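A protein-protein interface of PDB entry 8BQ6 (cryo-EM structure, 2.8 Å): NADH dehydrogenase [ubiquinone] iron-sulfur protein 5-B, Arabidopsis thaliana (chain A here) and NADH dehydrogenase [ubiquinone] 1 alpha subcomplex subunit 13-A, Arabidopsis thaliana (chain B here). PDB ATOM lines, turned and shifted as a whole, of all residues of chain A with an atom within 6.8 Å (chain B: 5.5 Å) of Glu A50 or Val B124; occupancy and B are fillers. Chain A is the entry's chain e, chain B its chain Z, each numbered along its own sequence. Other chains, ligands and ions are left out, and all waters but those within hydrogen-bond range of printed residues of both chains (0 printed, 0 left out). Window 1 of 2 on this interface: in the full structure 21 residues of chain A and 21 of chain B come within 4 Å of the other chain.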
ATOM      1  N   GLU A  39     -18.148 -35.144  10.363  1.00  0.00           N
ATOM      2  CA  GLU A  39     -17.365 -34.708   9.216  1.00  0.00           C
ATOM      3  C   GLU A  39     -16.148 -33.903   9.644  1.00  0.00           C
ATOM      4  O   GLU A  39     -15.172 -33.843   8.898  1.00  0.00           O
ATOM      5  CB  GLU A  39     -18.217 -33.918   8.226  1.00  0.00           C
ATOM      6  CG  GLU A  39     -18.995 -32.775   8.801  1.00  0.00           C
ATOM      7  CD  GLU A  39     -20.248 -32.518   8.004  1.00  0.00           C
ATOM      8  OE1 GLU A  39     -20.743 -31.372   8.015  1.00  0.00           O
ATOM      9  OE2 GLU A  39     -20.727 -33.467   7.350  1.00  0.00           O
ATOM     10  N   ASP A  40     -16.158 -33.323  10.846  1.00  0.00           N
ATOM     11  CA  ASP A  40     -14.930 -32.746  11.392  1.00  0.00           C
ATOM     12  C   ASP A  40     -13.869 -33.820  11.593  1.00  0.00           C
ATOM     13  O   ASP A  40     -12.699 -33.637  11.232  1.00  0.00           O
ATOM     14  CB  ASP A  40     -15.223 -32.052  12.718  1.00  0.00           C
ATOM     15  CG  ASP A  40     -15.602 -30.606  12.545  1.00  0.00           C
ATOM     16  OD1 ASP A  40     -16.806 -30.325  12.409  1.00  0.00           O
ATOM     17  OD2 ASP A  40     -14.703 -29.747  12.566  1.00  0.00           O
ATOM     18  N   GLU A  43     -12.714 -35.051   8.170  1.00  0.00           N
ATOM     19  CA  GLU A  43     -11.877 -34.010   7.590  1.00  0.00           C
ATOM     20  C   GLU A  43     -10.478 -34.023   8.189  1.00  0.00           C
ATOM     21  O   GLU A  43      -9.486 -33.905   7.462  1.00  0.00           O
ATOM     22  CB  GLU A  43     -12.540 -32.649   7.800  1.00  0.00           C
ATOM     23  CG  GLU A  43     -11.700 -31.471   7.358  1.00  0.00           C
ATOM     24  CD  GLU A  43     -11.405 -31.492   5.879  1.00  0.00           C
ATOM     25  OE1 GLU A  43     -12.253 -31.985   5.110  1.00  0.00           O
ATOM     26  OE2 GLU A  43     -10.323 -31.015   5.482  1.00  0.00           O
ATOM     27  N   HIS A  47      -8.271 -34.552   5.227  1.00  0.00           N
ATOM     28  CA  HIS A  47      -8.098 -33.192   4.701  1.00  0.00           C
ATOM     29  C   HIS A  47      -8.693 -33.044   3.308  1.00  0.00           C
ATOM     30  O   HIS A  47      -8.103 -32.402   2.437  1.00  0.00           O
ATOM     31  CB  HIS A  47      -6.628 -32.766   4.666  1.00  0.00           C
ATOM     32  CG  HIS A  47      -5.837 -33.201   5.856  1.00  0.00           C
ATOM     33  ND1 HIS A  47      -5.979 -32.620   7.096  1.00  0.00           N
ATOM     34  CD2 HIS A  47      -4.890 -34.157   5.993  1.00  0.00           C
ATOM     35  CE1 HIS A  47      -5.153 -33.200   7.948  1.00  0.00           C
ATOM     36  NE2 HIS A  47      -4.481 -34.137   7.304  1.00  0.00           N
ATOM     37  N   SER A  48      -9.853 -33.651   3.076  1.00  0.00           N
ATOM     38  CA  SER A  48     -10.433 -33.638   1.739  1.00  0.00           C
ATOM     39  C   SER A  48     -10.916 -32.244   1.355  1.00  0.00           C
ATOM     40  O   SER A  48     -10.603 -31.743   0.268  1.00  0.00           O
ATOM     41  CB  SER A  48     -11.578 -34.643   1.668  1.00  0.00           C
ATOM     42  OG  SER A  48     -11.111 -35.965   1.835  1.00  0.00           O
ATOM     43  N   LYS A  49     -11.678 -31.598   2.239  1.00  0.00           N
ATOM     44  CA  LYS A  49     -12.281 -30.317   1.889  1.00  0.00           C
ATOM     45  C   LYS A  49     -11.241 -29.206   1.848  1.00  0.00           C
ATOM     46  O   LYS A  49     -11.313 -28.310   0.997  1.00  0.00           O
ATOM     47  CB  LYS A  49     -13.396 -29.980   2.875  1.00  0.00           C
ATOM     48  CG  LYS A  49     -14.623 -30.853   2.716  1.00  0.00           C
ATOM     49  CD  LYS A  49     -15.702 -30.502   3.722  1.00  0.00           C
ATOM     50  CE  LYS A  49     -15.123 -30.224   5.091  1.00  0.00           C
ATOM     51  NZ  LYS A  49     -15.006 -31.482   5.861  1.00  0.00           N
ATOM     52  N   GLU A  50     -10.262 -29.256   2.753  1.00  0.00           N
ATOM     53  CA  GLU A  50      -9.166 -28.291   2.735  1.00  0.00           C
ATOM     54  C   GLU A  50      -8.397 -28.354   1.421  1.00  0.00           C
ATOM     55  O   GLU A  50      -8.117 -27.322   0.793  1.00  0.00           O
ATOM     56  CB  GLU A  50      -8.228 -28.562   3.909  1.00  0.00           C
ATOM     57  CG  GLU A  50      -7.484 -27.349   4.420  1.00  0.00           C
ATOM     58  CD  GLU A  50      -6.291 -27.722   5.282  1.00  0.00           C
ATOM     59  OE1 GLU A  50      -6.489 -28.331   6.355  1.00  0.00           O
ATOM     60  OE2 GLU A  50      -5.153 -27.401   4.888  1.00  0.00           O
ATOM     61  N   PHE A  51      -8.036 -29.566   0.995  1.00  0.00           N
ATOM     62  CA  PHE A  51      -7.264 -29.713  -0.232  1.00  0.00           C
ATOM     63  C   PHE A  51      -8.105 -29.371  -1.452  1.00  0.00           C
ATOM     64  O   PHE A  51      -7.594 -28.809  -2.423  1.00  0.00           O
ATOM     65  CB  PHE A  51      -6.704 -31.129  -0.342  1.00  0.00           C
ATOM     66  CG  PHE A  51      -5.616 -31.423   0.643  1.00  0.00           C
ATOM     67  CD1 PHE A  51      -5.047 -30.408   1.389  1.00  0.00           C
ATOM     68  CD2 PHE A  51      -5.157 -32.713   0.820  1.00  0.00           C
ATOM     69  CE1 PHE A  51      -4.053 -30.674   2.292  1.00  0.00           C
ATOM     70  CE2 PHE A  51      -4.159 -32.985   1.723  1.00  0.00           C
ATOM     71  CZ  PHE A  51      -3.607 -31.966   2.461  1.00  0.00           C
ATOM     72  N   GLN A  52      -9.397 -29.692  -1.416  1.00  0.00           N
ATOM     73  CA  GLN A  52     -10.282 -29.292  -2.503  1.00  0.00           C
ATOM     74  C   GLN A  52     -10.334 -27.774  -2.642  1.00  0.00           C
ATOM     75  O   GLN A  52     -10.258 -27.239  -3.754  1.00  0.00           O
ATOM     76  CB  GLN A  52     -11.675 -29.860  -2.264  1.00  0.00           C
ATOM     77  CG  GLN A  52     -12.202 -30.687  -3.406  1.00  0.00           C
ATOM     78  CD  GLN A  52     -13.548 -31.289  -3.095  1.00  0.00           C
ATOM     79  OE1 GLN A  52     -13.790 -31.748  -1.979  1.00  0.00           O
ATOM     80  NE2 GLN A  52     -14.438 -31.295  -4.080  1.00  0.00           N
ATOM     81  N   ARG A  53     -10.452 -27.063  -1.519  1.00  0.00           N
ATOM     82  CA  ARG A  53     -10.480 -25.605  -1.565  1.00  0.00           C
ATOM     83  C   ARG A  53      -9.159 -25.028  -2.078  1.00  0.00           C
ATOM     84  O   ARG A  53      -9.148 -24.091  -2.896  1.00  0.00           O
ATOM     85  CB  ARG A  53     -10.805 -25.064  -0.178  1.00  0.00           C
ATOM     86  CG  ARG A  53     -10.364 -23.646   0.049  1.00  0.00           C
ATOM     87  CD  ARG A  53     -10.093 -23.399   1.519  1.00  0.00           C
ATOM     88  NE  ARG A  53     -10.181 -21.988   1.871  1.00  0.00           N
ATOM     89  CZ  ARG A  53     -11.281 -21.254   1.762  1.00  0.00           C
ATOM     90  NH1 ARG A  53     -12.414 -21.763   1.302  1.00  0.00           N
ATOM     91  NH2 ARG A  53     -11.250 -19.980   2.137  1.00  0.00           N
ATOM     92  N   ARG A  54      -8.033 -25.569  -1.611  1.00  0.00           N
ATOM     93  CA  ARG A  54      -6.748 -25.081  -2.104  1.00  0.00           C
ATOM     94  C   ARG A  54      -6.561 -25.386  -3.584  1.00  0.00           C
ATOM     95  O   ARG A  54      -5.930 -24.605  -4.310  1.00  0.00           O
ATOM     96  CB  ARG A  54      -5.606 -25.668  -1.284  1.00  0.00           C
ATOM     97  CG  ARG A  54      -5.388 -24.928   0.010  1.00  0.00           C
ATOM     98  CD  ARG A  54      -4.782 -25.820   1.057  1.00  0.00           C
ATOM     99  NE  ARG A  54      -3.327 -25.777   1.032  1.00  0.00           N
ATOM    100  CZ  ARG A  54      -2.557 -26.365   1.935  1.00  0.00           C
ATOM    101  NH1 ARG A  54      -3.075 -27.046   2.943  1.00  0.00           N
ATOM    102  NH2 ARG A  54      -1.236 -26.266   1.826  1.00  0.00           N
ATOM    103  N   ASN A  55      -7.113 -26.502  -4.056  1.00  0.00           N
ATOM    104  CA  ASN A  55      -7.053 -26.791  -5.480  1.00  0.00           C
ATOM    105  C   ASN A  55      -7.925 -25.831  -6.271  1.00  0.00           C
ATOM    106  O   ASN A  55      -7.573 -25.474  -7.397  1.00  0.00           O
ATOM    107  CB  ASN A  55      -7.460 -28.236  -5.744  1.00  0.00           C
ATOM    108  CG  ASN A  55      -6.425 -29.225  -5.252  1.00  0.00           C
ATOM    109  OD1 ASN A  55      -5.298 -28.852  -4.929  1.00  0.00           O
ATOM    110  ND2 ASN A  55      -6.794 -30.495  -5.217  1.00  0.00           N
ATOM    111  N   GLU B 122     -11.603 -19.283   4.986  1.00  0.00           N
ATOM    112  CA  GLU B 122     -12.707 -19.976   5.634  1.00  0.00           C
ATOM    113  C   GLU B 122     -12.198 -21.223   6.352  1.00  0.00           C
ATOM    114  O   GLU B 122     -11.342 -21.946   5.833  1.00  0.00           O
ATOM    115  CB  GLU B 122     -13.783 -20.337   4.602  1.00  0.00           C
ATOM    116  CG  GLU B 122     -14.788 -21.387   5.065  1.00  0.00           C
ATOM    117  CD  GLU B 122     -16.197 -21.171   4.518  1.00  0.00           C
ATOM    118  OE1 GLU B 122     -16.483 -21.581   3.372  1.00  0.00           O
ATOM    119  OE2 GLU B 122     -17.029 -20.598   5.248  1.00  0.00           O
ATOM    120  N   ASN B 123     -12.706 -21.459   7.562  1.00  0.00           N
ATOM    121  CA  ASN B 123     -12.338 -22.642   8.332  1.00  0.00           C
ATOM    122  C   ASN B 123     -13.176 -23.832   7.878  1.00  0.00           C
ATOM    123  O   ASN B 123     -14.401 -23.830   8.040  1.00  0.00           O
ATOM    124  CB  ASN B 123     -12.542 -22.384   9.825  1.00  0.00           C
ATOM    125  CG  ASN B 123     -11.762 -23.348  10.705  1.00  0.00           C
ATOM    126  OD1 ASN B 123     -11.493 -24.484  10.318  1.00  0.00           O
ATOM    127  ND2 ASN B 123     -11.417 -22.904  11.907  1.00  0.00           N
ATOM    128  N   VAL B 124     -12.522 -24.850   7.315  1.00  0.00           N
ATOM    129  CA  VAL B 124     -13.253 -26.025   6.853  1.00  0.00           C
ATOM    130  C   VAL B 124     -13.838 -26.843   7.998  1.00  0.00           C
ATOM    131  O   VAL B 124     -14.700 -27.694   7.756  1.00  0.00           O
ATOM    132  CB  VAL B 124     -12.377 -26.940   5.981  1.00  0.00           C
ATOM    133  CG1 VAL B 124     -12.129 -26.305   4.621  1.00  0.00           C
ATOM    134  CG2 VAL B 124     -11.062 -27.248   6.684  1.00  0.00           C
ATOM    135  N   TYR B 125     -13.403 -26.615   9.234  1.00  0.00           N
ATOM    136  CA  TYR B 125     -13.928 -27.368  10.366  1.00  0.00           C
ATOM    137  C   TYR B 125     -15.165 -26.685  10.934  1.00  0.00           C
ATOM    138  O   TYR B 125     -15.159 -25.475  11.177  1.00  0.00           O
ATOM    139  CB  TYR B 125     -12.855 -27.524  11.441  1.00  0.00           C
ATOM    140  CG  TYR B 125     -11.755 -28.446  10.993  1.00  0.00           C
ATOM    141  CD1 TYR B 125     -11.918 -29.824  11.045  1.00  0.00           C
ATOM    142  CD2 TYR B 125     -10.573 -27.945  10.476  1.00  0.00           C
ATOM    143  CE1 TYR B 125     -10.929 -30.671  10.616  1.00  0.00           C
ATOM    144  CE2 TYR B 125      -9.577 -28.784  10.046  1.00  0.00           C
ATOM    145  CZ  TYR B 125      -9.759 -30.145  10.117  1.00  0.00           C
ATOM    146  OH  TYR B 125      -8.761 -30.980   9.686  1.00  0.00           O
ATOM    147  N   ASN B 126     -16.234 -27.464  11.132  1.00  0.00           N
ATOM    148  CA  ASN B 126     -17.482 -26.887  11.624  1.00  0.00           C
ATOM    149  C   ASN B 126     -17.324 -26.370  13.048  1.00  0.00           C
ATOM    150  O   ASN B 126     -17.887 -25.328  13.402  1.00  0.00           O
ATOM    151  CB  ASN B 126     -18.617 -27.908  11.540  1.00  0.00           C
ATOM    152  CG  ASN B 126     -18.900 -28.353  10.116  1.00  0.00           C
ATOM    153  OD1 ASN B 126     -18.777 -29.531   9.783  1.00  0.00           O
ATOM    154  ND2 ASN B 126     -19.252 -27.403   9.261  1.00  0.00           N
ATOM    155  N   PRO B 132      -3.423 -26.344  12.254  1.00  0.00           N
ATOM    156  CA  PRO B 132      -2.387 -25.874  11.342  1.00  0.00           C
ATOM    157  C   PRO B 132      -2.727 -26.266   9.920  1.00  0.00           C
ATOM    158  O   PRO B 132      -3.448 -27.256   9.686  1.00  0.00           O
ATOM    159  CB  PRO B 132      -1.120 -26.585  11.841  1.00  0.00           C
ATOM    160  CG  PRO B 132      -1.468 -27.213  13.142  1.00  0.00           C
ATOM    161  CD  PRO B 132      -2.941 -27.365  13.197  1.00  0.00           C
ATOM    162  N   PRO B 133      -2.264 -25.501   8.935  1.00  0.00           N
ATOM    163  CA  PRO B 133      -2.602 -25.833   7.546  1.00  0.00           C
ATOM    164  C   PRO B 133      -1.962 -27.152   7.141  1.00  0.00           C
ATOM    165  O   PRO B 133      -0.782 -27.395   7.400  1.00  0.00           O
ATOM    166  CB  PRO B 133      -2.037 -24.652   6.745  1.00  0.00           C
ATOM    167  CG  PRO B 133      -1.632 -23.622   7.756  1.00  0.00           C
ATOM    168  CD  PRO B 133      -1.355 -24.349   9.023  1.00  0.00           C
ATOM    169  N   ALA B 134      -2.759 -28.011   6.514  1.00  0.00           N
ATOM    170  CA  ALA B 134      -2.274 -29.314   6.092  1.00  0.00           C
ATOM    171  C   ALA B 134      -1.275 -29.166   4.951  1.00  0.00           C
ATOM    172  O   ALA B 134      -1.402 -28.289   4.093  1.00  0.00           O
ATOM    173  CB  ALA B 134      -3.438 -30.204   5.664  1.00  0.00           C
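Hydrophobic or aromatic side chains of chain B within 4 Å of the printed part of chain A: Val B124, Tyr B125 and Ala B134.
Among the printed residues, 12 pairs touch across the chains.
The guanidinium group (NH1) of Arg A54 is in salt-bridge range of the side-chain carboxylate (OE2) of Glu A50 (2.9 Å).
OE2 of Glu A43 is in hydrogen-bond range of N of Glu A50 (3.2 Å).
The side-chain amide nitrogen (ND2) of Asn A55 sits close to the backbone carbonyl oxygen (O) of Phe A51, 3.4 Å away.
The side-chain amino group of Lys A49 is in salt-bridge range of the side-chain carboxylate of Glu A43 (2.9 Å).
The side-chain amide oxygen (OD1) of Asn B123 sits at hydrogen-bond distance from the backbone NH (N) of Tyr B125, 3.1 Å away.
Among the printed residues, merely in contact across the chains: Asp A40 with Tyr B125 (3.1 Å), Glu A43 with Tyr B125 (3.4 Å), His A47 with Ala B134 (3.8 Å), Lys A49 with Val B124 (3.7 Å), Glu A50 with Val B124 (3.96 Å), Glu A50 with Pro B133 (3.9 Å) and Phe A51 with Ala B134 (3.5 Å).
Of the printed residues of chain B, Glu A39 touches Asn B126 (3.2 Å).
Glu A50 touches just these residues of chain B: Val B124, Pro B133 and Ala B134.
Gln A52 touches none of the printed residues of chain B.
Printed residues of chain B within 4 Å of Arg A53: Glu B122.
Of the printed residues of chain B, Arg A54 touches Ala B134 (2.4 Å).
Printed residues of chain A within 4 Å of Tyr B125: Asp A40 (3.1 Å) and Glu A43 (3.4 Å).
Of the printed residues of chain A, Pro B133 touches Glu A50 (3.9 Å).
The nearest residue of chain B that does not touch Glu A50 is Pro B132 (4.6 Å).
The nearest residue of chain A that does not touch Val B124 is Glu A43 (4.02 Å).
O of Ala B134 sits at hydrogen-bond distance from NH2 of Arg A54, 3.0 Å away.
The side-chain carboxylate (OE2) of Glu A50 sits at hydrogen-bond distance from the backbone NH (N) of Ala B134 (3.0 Å).
The guanidinium group of Arg A53 sits close to the backbone NH of Glu B122 (3.0 Å).
The side-chain carboxylate of Asp A40 sits at hydrogen-bond distance from the backbone NH of Asn B126 (3.1 Å).
The side-chain amide oxygen (OD1) of Asn B126 sits close to the side-chain carboxylate (OE1) of Glu A39.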
